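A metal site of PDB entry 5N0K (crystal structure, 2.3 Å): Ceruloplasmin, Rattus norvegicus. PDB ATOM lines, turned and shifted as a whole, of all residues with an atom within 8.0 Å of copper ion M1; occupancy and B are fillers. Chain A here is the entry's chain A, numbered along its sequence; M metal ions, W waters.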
ATOM      1  N   HIS A 120      -8.814  19.147  24.254  1.00  0.00           N
ATOM      2  CA  HIS A 120      -9.490  20.411  24.172  1.00  0.00           C
ATOM      3  C   HIS A 120     -10.671  20.356  23.188  1.00  0.00           C
ATOM      4  O   HIS A 120     -10.453  20.079  22.025  1.00  0.00           O
ATOM      5  CB  HIS A 120      -8.523  21.452  23.673  1.00  0.00           C
ATOM      6  CG  HIS A 120      -9.171  22.742  23.457  1.00  0.00           C
ATOM      7  ND1 HIS A 120      -9.839  23.369  24.478  1.00  0.00           N
ATOM      8  CD2 HIS A 120      -9.370  23.485  22.363  1.00  0.00           C
ATOM      9  CE1 HIS A 120     -10.384  24.492  24.027  1.00  0.00           C
ATOM     10  NE2 HIS A 120     -10.117  24.570  22.748  1.00  0.00           N
ATOM     11  N   ALA A 121     -11.878  20.676  23.655  1.00  0.00           N
ATOM     12  CA  ALA A 121     -13.127  20.507  22.849  1.00  0.00           C
ATOM     13  C   ALA A 121     -13.648  21.838  22.317  1.00  0.00           C
ATOM     14  O   ALA A 121     -13.714  22.781  23.078  1.00  0.00           O
ATOM     15  CB  ALA A 121     -14.210  19.842  23.668  1.00  0.00           C
ATOM     16  N   HIS A 122     -14.025  21.871  21.040  1.00  0.00           N
ATOM     17  CA  HIS A 122     -14.768  22.985  20.418  1.00  0.00           C
ATOM     18  C   HIS A 122     -16.285  23.107  20.676  1.00  0.00           C
ATOM     19  O   HIS A 122     -16.828  24.192  20.891  1.00  0.00           O
ATOM     20  CB  HIS A 122     -14.575  22.982  18.893  1.00  0.00           C
ATOM     21  CG  HIS A 122     -13.263  23.552  18.455  1.00  0.00           C
ATOM     22  ND1 HIS A 122     -13.157  24.608  17.574  1.00  0.00           N
ATOM     23  CD2 HIS A 122     -11.999  23.238  18.828  1.00  0.00           C
ATOM     24  CE1 HIS A 122     -11.887  24.887  17.399  1.00  0.00           C
ATOM     25  NE2 HIS A 122     -11.168  24.084  18.170  1.00  0.00           N
ATOM     26  N   ILE A 177     -14.960  19.691  16.772  1.00  0.00           N
ATOM     27  CA  ILE A 177     -13.702  18.927  16.859  1.00  0.00           C
ATOM     28  C   ILE A 177     -13.150  18.999  18.256  1.00  0.00           C
ATOM     29  O   ILE A 177     -13.627  19.811  19.087  1.00  0.00           O
ATOM     30  CB  ILE A 177     -12.637  19.457  15.876  1.00  0.00           C
ATOM     31  CG1 ILE A 177     -12.338  20.936  16.124  1.00  0.00           C
ATOM     32  CG2 ILE A 177     -13.082  19.228  14.443  1.00  0.00           C
ATOM     33  CD1 ILE A 177     -11.164  21.426  15.327  1.00  0.00           C
ATOM     34  N   TYR A 178     -12.179  18.122  18.518  1.00  0.00           N
ATOM     35  CA  TYR A 178     -11.346  18.225  19.724  1.00  0.00           C
ATOM     36  C   TYR A 178      -9.919  17.947  19.315  1.00  0.00           C
ATOM     37  O   TYR A 178      -9.674  17.250  18.309  1.00  0.00           O
ATOM     38  CB  TYR A 178     -11.812  17.302  20.876  1.00  0.00           C
ATOM     39  CG  TYR A 178     -11.699  15.840  20.580  1.00  0.00           C
ATOM     40  CD1 TYR A 178     -10.500  15.157  20.734  1.00  0.00           C
ATOM     41  CD2 TYR A 178     -12.827  15.121  20.150  1.00  0.00           C
ATOM     42  CE1 TYR A 178     -10.402  13.806  20.458  1.00  0.00           C
ATOM     43  CE2 TYR A 178     -12.742  13.775  19.843  1.00  0.00           C
ATOM     44  CZ  TYR A 178     -11.543  13.127  20.009  1.00  0.00           C
ATOM     45  OH  TYR A 178     -11.493  11.799  19.690  1.00  0.00           O
ATOM     46  N   HIS A 179      -8.994  18.502  20.082  1.00  0.00           N
ATOM     47  CA  HIS A 179      -7.583  18.307  19.802  1.00  0.00           C
ATOM     48  C   HIS A 179      -6.690  18.737  20.994  1.00  0.00           C
ATOM     49  O   HIS A 179      -7.138  19.386  21.931  1.00  0.00           O
ATOM     50  CB  HIS A 179      -7.207  19.053  18.522  1.00  0.00           C
ATOM     51  CG  HIS A 179      -7.417  20.519  18.629  1.00  0.00           C
ATOM     52  ND1 HIS A 179      -6.443  21.356  19.099  1.00  0.00           N
ATOM     53  CD2 HIS A 179      -8.502  21.291  18.389  1.00  0.00           C
ATOM     54  CE1 HIS A 179      -6.889  22.589  19.123  1.00  0.00           C
ATOM     55  NE2 HIS A 179      -8.125  22.574  18.701  1.00  0.00           N
ATOM     56  N   SER A 180      -5.426  18.358  20.951  1.00  0.00           N
ATOM     57  CA  SER A 180      -4.522  18.729  22.034  1.00  0.00           C
ATOM     58  C   SER A 180      -4.108  20.173  21.841  1.00  0.00           C
ATOM     59  O   SER A 180      -4.060  20.673  20.711  1.00  0.00           O
ATOM     60  CB  SER A 180      -3.305  17.796  22.070  1.00  0.00           C
ATOM     61  OG  SER A 180      -2.383  18.224  23.044  1.00  0.00           O
ATOM     62  N   HIS A 181      -3.792  20.850  22.932  1.00  0.00           N
ATOM     63  CA  HIS A 181      -3.564  22.286  22.897  1.00  0.00           C
ATOM     64  C   HIS A 181      -2.503  22.738  23.886  1.00  0.00           C
ATOM     65  O   HIS A 181      -2.691  23.682  24.669  1.00  0.00           O
ATOM     66  CB  HIS A 181      -4.880  22.995  23.128  1.00  0.00           C
ATOM     67  CG  HIS A 181      -4.899  24.384  22.605  1.00  0.00           C
ATOM     68  ND1 HIS A 181      -3.995  25.334  23.004  1.00  0.00           N
ATOM     69  CD2 HIS A 181      -5.723  24.994  21.728  1.00  0.00           C
ATOM     70  CE1 HIS A 181      -4.240  26.477  22.385  1.00  0.00           C
ATOM     71  NE2 HIS A 181      -5.288  26.290  21.603  1.00  0.00           N
ATOM     72  N   ALA A 184      -0.998  23.889  19.998  1.00  0.00           N
ATOM     73  CA  ALA A 184      -2.039  23.218  19.246  1.00  0.00           C
ATOM     74  C   ALA A 184      -1.584  22.825  17.845  1.00  0.00           C
ATOM     75  O   ALA A 184      -1.784  21.682  17.459  1.00  0.00           O
ATOM     76  CB  ALA A 184      -3.331  24.049  19.193  1.00  0.00           C
ATOM     77  N   ILE A 188      -1.465  18.886  16.740  1.00  0.00           N
ATOM     78  CA  ILE A 188      -2.407  18.421  15.709  1.00  0.00           C
ATOM     79  C   ILE A 188      -1.624  17.738  14.605  1.00  0.00           C
ATOM     80  O   ILE A 188      -2.015  16.676  14.107  1.00  0.00           O
ATOM     81  CB  ILE A 188      -3.263  19.593  15.121  1.00  0.00           C
ATOM     82  CG1 ILE A 188      -4.270  20.094  16.161  1.00  0.00           C
ATOM     83  CG2 ILE A 188      -3.970  19.163  13.843  1.00  0.00           C
ATOM     84  CD1 ILE A 188      -4.799  21.499  15.902  1.00  0.00           C
ATOM     85  N   ILE A 193      -6.151  14.904  16.992  1.00  0.00           N
ATOM     86  CA  ILE A 193      -7.347  15.598  16.524  1.00  0.00           C
ATOM     87  C   ILE A 193      -8.404  14.545  16.358  1.00  0.00           C
ATOM     88  O   ILE A 193      -8.116  13.415  15.918  1.00  0.00           O
ATOM     89  CB  ILE A 193      -7.058  16.355  15.184  1.00  0.00           C
ATOM     90  CG1 ILE A 193      -8.303  17.012  14.556  1.00  0.00           C
ATOM     91  CG2 ILE A 193      -6.438  15.422  14.148  1.00  0.00           C
ATOM     92  CD1 ILE A 193      -8.658  18.380  15.073  1.00  0.00           C
ATOM     93  N   MET A 287      -8.082  21.217   8.333  1.00  0.00           N
ATOM     94  CA  MET A 287      -7.093  21.483   9.361  1.00  0.00           C
ATOM     95  C   MET A 287      -5.751  21.809   8.741  1.00  0.00           C
ATOM     96  O   MET A 287      -5.347  21.195   7.769  1.00  0.00           O
ATOM     97  CB  MET A 287      -6.964  20.234  10.257  1.00  0.00           C
ATOM     98  CG  MET A 287      -6.379  20.494  11.618  1.00  0.00           C
ATOM     99  SD  MET A 287      -7.229  21.697  12.690  1.00  0.00           S
ATOM    100  CE  MET A 287      -8.904  21.169  12.607  1.00  0.00           C
ATOM    101  N   PRO A 317      -8.257  25.799   7.603  1.00  0.00           N
ATOM    102  CA  PRO A 317      -7.940  25.304   8.952  1.00  0.00           C
ATOM    103  C   PRO A 317      -9.062  25.544   9.996  1.00  0.00           C
ATOM    104  O   PRO A 317      -9.347  26.676  10.386  1.00  0.00           O
ATOM    105  CB  PRO A 317      -6.677  26.065   9.295  1.00  0.00           C
ATOM    106  CG  PRO A 317      -6.030  26.282   7.949  1.00  0.00           C
ATOM    107  CD  PRO A 317      -7.201  26.656   7.069  1.00  0.00           C
ATOM    108  N   ALA A 318      -9.654  24.451  10.439  1.00  0.00           N
ATOM    109  CA  ALA A 318     -10.735  24.366  11.394  1.00  0.00           C
ATOM    110  C   ALA A 318     -12.100  24.831  10.871  1.00  0.00           C
ATOM    111  O   ALA A 318     -13.043  25.009  11.660  1.00  0.00           O
ATOM    112  CB  ALA A 318     -10.369  25.014  12.727  1.00  0.00           C
ATOM    113  N   LEU A 320     -15.653  24.182   9.917  1.00  0.00           N
ATOM    114  CA  LEU A 320     -16.583  23.160  10.376  1.00  0.00           C
ATOM    115  C   LEU A 320     -17.839  23.257   9.553  1.00  0.00           C
ATOM    116  O   LEU A 320     -18.454  24.296   9.520  1.00  0.00           O
ATOM    117  CB  LEU A 320     -16.970  23.391  11.829  1.00  0.00           C
ATOM    118  CG  LEU A 320     -15.805  23.579  12.810  1.00  0.00           C
ATOM    119  CD1 LEU A 320     -16.344  24.047  14.168  1.00  0.00           C
ATOM    120  CD2 LEU A 320     -14.968  22.319  12.959  1.00  0.00           C
ATOM    121  N   HIS A 991     -11.511  31.678  15.867  1.00  0.00           N
ATOM    122  CA  HIS A 991     -11.971  30.793  16.904  1.00  0.00           C
ATOM    123  C   HIS A 991     -11.953  31.470  18.304  1.00  0.00           C
ATOM    124  O   HIS A 991     -10.938  32.031  18.746  1.00  0.00           O
ATOM    125  CB  HIS A 991     -11.061  29.585  16.894  1.00  0.00           C
ATOM    126  CG  HIS A 991     -11.383  28.616  17.959  1.00  0.00           C
ATOM    127  ND1 HIS A 991     -12.663  28.167  18.187  1.00  0.00           N
ATOM    128  CD2 HIS A 991     -10.618  28.084  18.940  1.00  0.00           C
ATOM    129  CE1 HIS A 991     -12.661  27.365  19.227  1.00  0.00           C
ATOM    130  NE2 HIS A 991     -11.430  27.307  19.703  1.00  0.00           N
ATOM    131  N   HIS A 993     -12.265  30.552  22.168  1.00  0.00           N
ATOM    132  CA  HIS A 993     -12.352  29.588  23.259  1.00  0.00           C
ATOM    133  C   HIS A 993     -13.448  30.057  24.170  1.00  0.00           C
ATOM    134  O   HIS A 993     -13.720  31.254  24.279  1.00  0.00           O
ATOM    135  CB  HIS A 993     -11.050  29.496  24.079  1.00  0.00           C
ATOM    136  CG  HIS A 993      -9.930  28.807  23.377  1.00  0.00           C
ATOM    137  ND1 HIS A 993      -9.100  27.904  24.009  1.00  0.00           N
ATOM    138  CD2 HIS A 993      -9.509  28.868  22.101  1.00  0.00           C
ATOM    139  CE1 HIS A 993      -8.214  27.458  23.145  1.00  0.00           C
ATOM    140  NE2 HIS A 993      -8.431  28.035  21.980  1.00  0.00           N
ATOM    141  N   ASP A1008     -18.192  27.855  16.322  1.00  0.00           N
ATOM    142  CA  ASP A1008     -17.112  28.563  17.033  1.00  0.00           C
ATOM    143  C   ASP A1008     -15.858  28.807  16.224  1.00  0.00           C
ATOM    144  O   ASP A1008     -14.839  29.206  16.768  1.00  0.00           O
ATOM    145  CB  ASP A1008     -16.783  27.888  18.380  1.00  0.00           C
ATOM    146  CG  ASP A1008     -16.139  26.553  18.220  1.00  0.00           C
ATOM    147  OD1 ASP A1008     -15.949  26.063  17.060  1.00  0.00           O
ATOM    148  OD2 ASP A1008     -15.775  26.018  19.292  1.00  0.00           O
ATOM    149  N   VAL A1009     -15.946  28.532  14.926  1.00  0.00           N
ATOM    150  CA  VAL A1009     -14.924  28.978  13.965  1.00  0.00           C
ATOM    151  C   VAL A1009     -15.662  29.721  12.839  1.00  0.00           C
ATOM    152  O   VAL A1009     -16.580  29.168  12.300  1.00  0.00           O
ATOM    153  CB  VAL A1009     -14.101  27.795  13.431  1.00  0.00           C
ATOM    154  CG1 VAL A1009     -13.138  28.234  12.334  1.00  0.00           C
ATOM    155  CG2 VAL A1009     -13.321  27.149  14.570  1.00  0.00           C
ATOM    156  N   HIS A1033      -8.200  33.498  18.618  1.00  0.00           N
ATOM    157  CA  HIS A1033      -7.123  33.409  17.645  1.00  0.00           C
ATOM    158  C   HIS A1033      -7.589  32.892  16.328  1.00  0.00           C
ATOM    159  O   HIS A1033      -8.615  32.201  16.235  1.00  0.00           O
ATOM    160  CB  HIS A1033      -5.978  32.534  18.162  1.00  0.00           C
ATOM    161  CG  HIS A1033      -6.344  31.093  18.324  1.00  0.00           C
ATOM    162  ND1 HIS A1033      -6.143  30.171  17.320  1.00  0.00           N
ATOM    163  CD2 HIS A1033      -6.871  30.419  19.355  1.00  0.00           C
ATOM    164  CE1 HIS A1033      -6.565  28.989  17.723  1.00  0.00           C
ATOM    165  NE2 HIS A1033      -7.001  29.116  18.957  1.00  0.00           N
ATOM    166  N   HIS A1035      -7.137  30.311  13.387  1.00  0.00           N
ATOM    167  CA  HIS A1035      -6.775  28.909  13.599  1.00  0.00           C
ATOM    168  C   HIS A1035      -5.764  28.380  12.590  1.00  0.00           C
ATOM    169  O   HIS A1035      -5.452  27.183  12.606  1.00  0.00           O
ATOM    170  CB  HIS A1035      -8.017  28.046  13.600  1.00  0.00           C
ATOM    171  CG  HIS A1035      -7.964  26.871  14.527  1.00  0.00           C
ATOM    172  ND1 HIS A1035      -7.122  25.804  14.323  1.00  0.00           N
ATOM    173  CD2 HIS A1035      -8.731  26.555  15.594  1.00  0.00           C
ATOM    174  CE1 HIS A1035      -7.333  24.899  15.260  1.00  0.00           C
ATOM    175  NE2 HIS A1035      -8.301  25.333  16.045  1.00  0.00           N
ATOM    176  N   ILE A1040      -1.117  31.609  14.005  1.00  0.00           N
ATOM    177  CA  ILE A1040      -1.034  31.489  15.490  1.00  0.00           C
ATOM    178  C   ILE A1040       0.439  31.672  15.885  1.00  0.00           C
ATOM    179  O   ILE A1040       0.735  32.475  16.752  1.00  0.00           O
ATOM    180  CB  ILE A1040      -1.527  30.168  16.158  1.00  0.00           C
ATOM    181  CG1 ILE A1040      -2.706  29.578  15.415  1.00  0.00           C
ATOM    182  CG2 ILE A1040      -1.931  30.441  17.622  1.00  0.00           C
ATOM    183  CD1 ILE A1040      -3.418  28.404  16.092  1.00  0.00           C
HETATM  184 CU    CU M   1      -9.185  24.266  17.659  1.00  0.00          CU
HETATM  185 CU    CU M   2     -10.882  25.902  21.069  1.00  0.00          CU
HETATM  186 CU    CU M   3      -6.999  27.425  20.530  1.00  0.00          CU
HETATM  187  O   HOH W   1      -8.558  25.704  19.109  1.00  0.00           O
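O of Ile 177 sits at hydrogen-bond distance from N of His 122 (2.9 Å). A ring nitrogen (ND1) of His 122 lies within hydrogen-bond range of the side-chain carboxylate (OD1) of Asp 1008 (3.2 Å). The backbone carbonyl oxygen (O) of His 179 sits at hydrogen-bond distance from the backbone NH (N) of His 120 (2.9 Å).
Along chain A the residues within 4 Å of copper ion M1 span positions 122 to 1035.
A ring nitrogen (NE2) of His 122 is bound to copper ion M1 (2.1 Å). Copper ion M1 is bound by NE2 of His 1035, at 2.1 Å. Copper ion M1 is bound by water W1, 2.1 Å away. Copper ion M1 is bound by NE2 of His 179 (2.3 Å).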
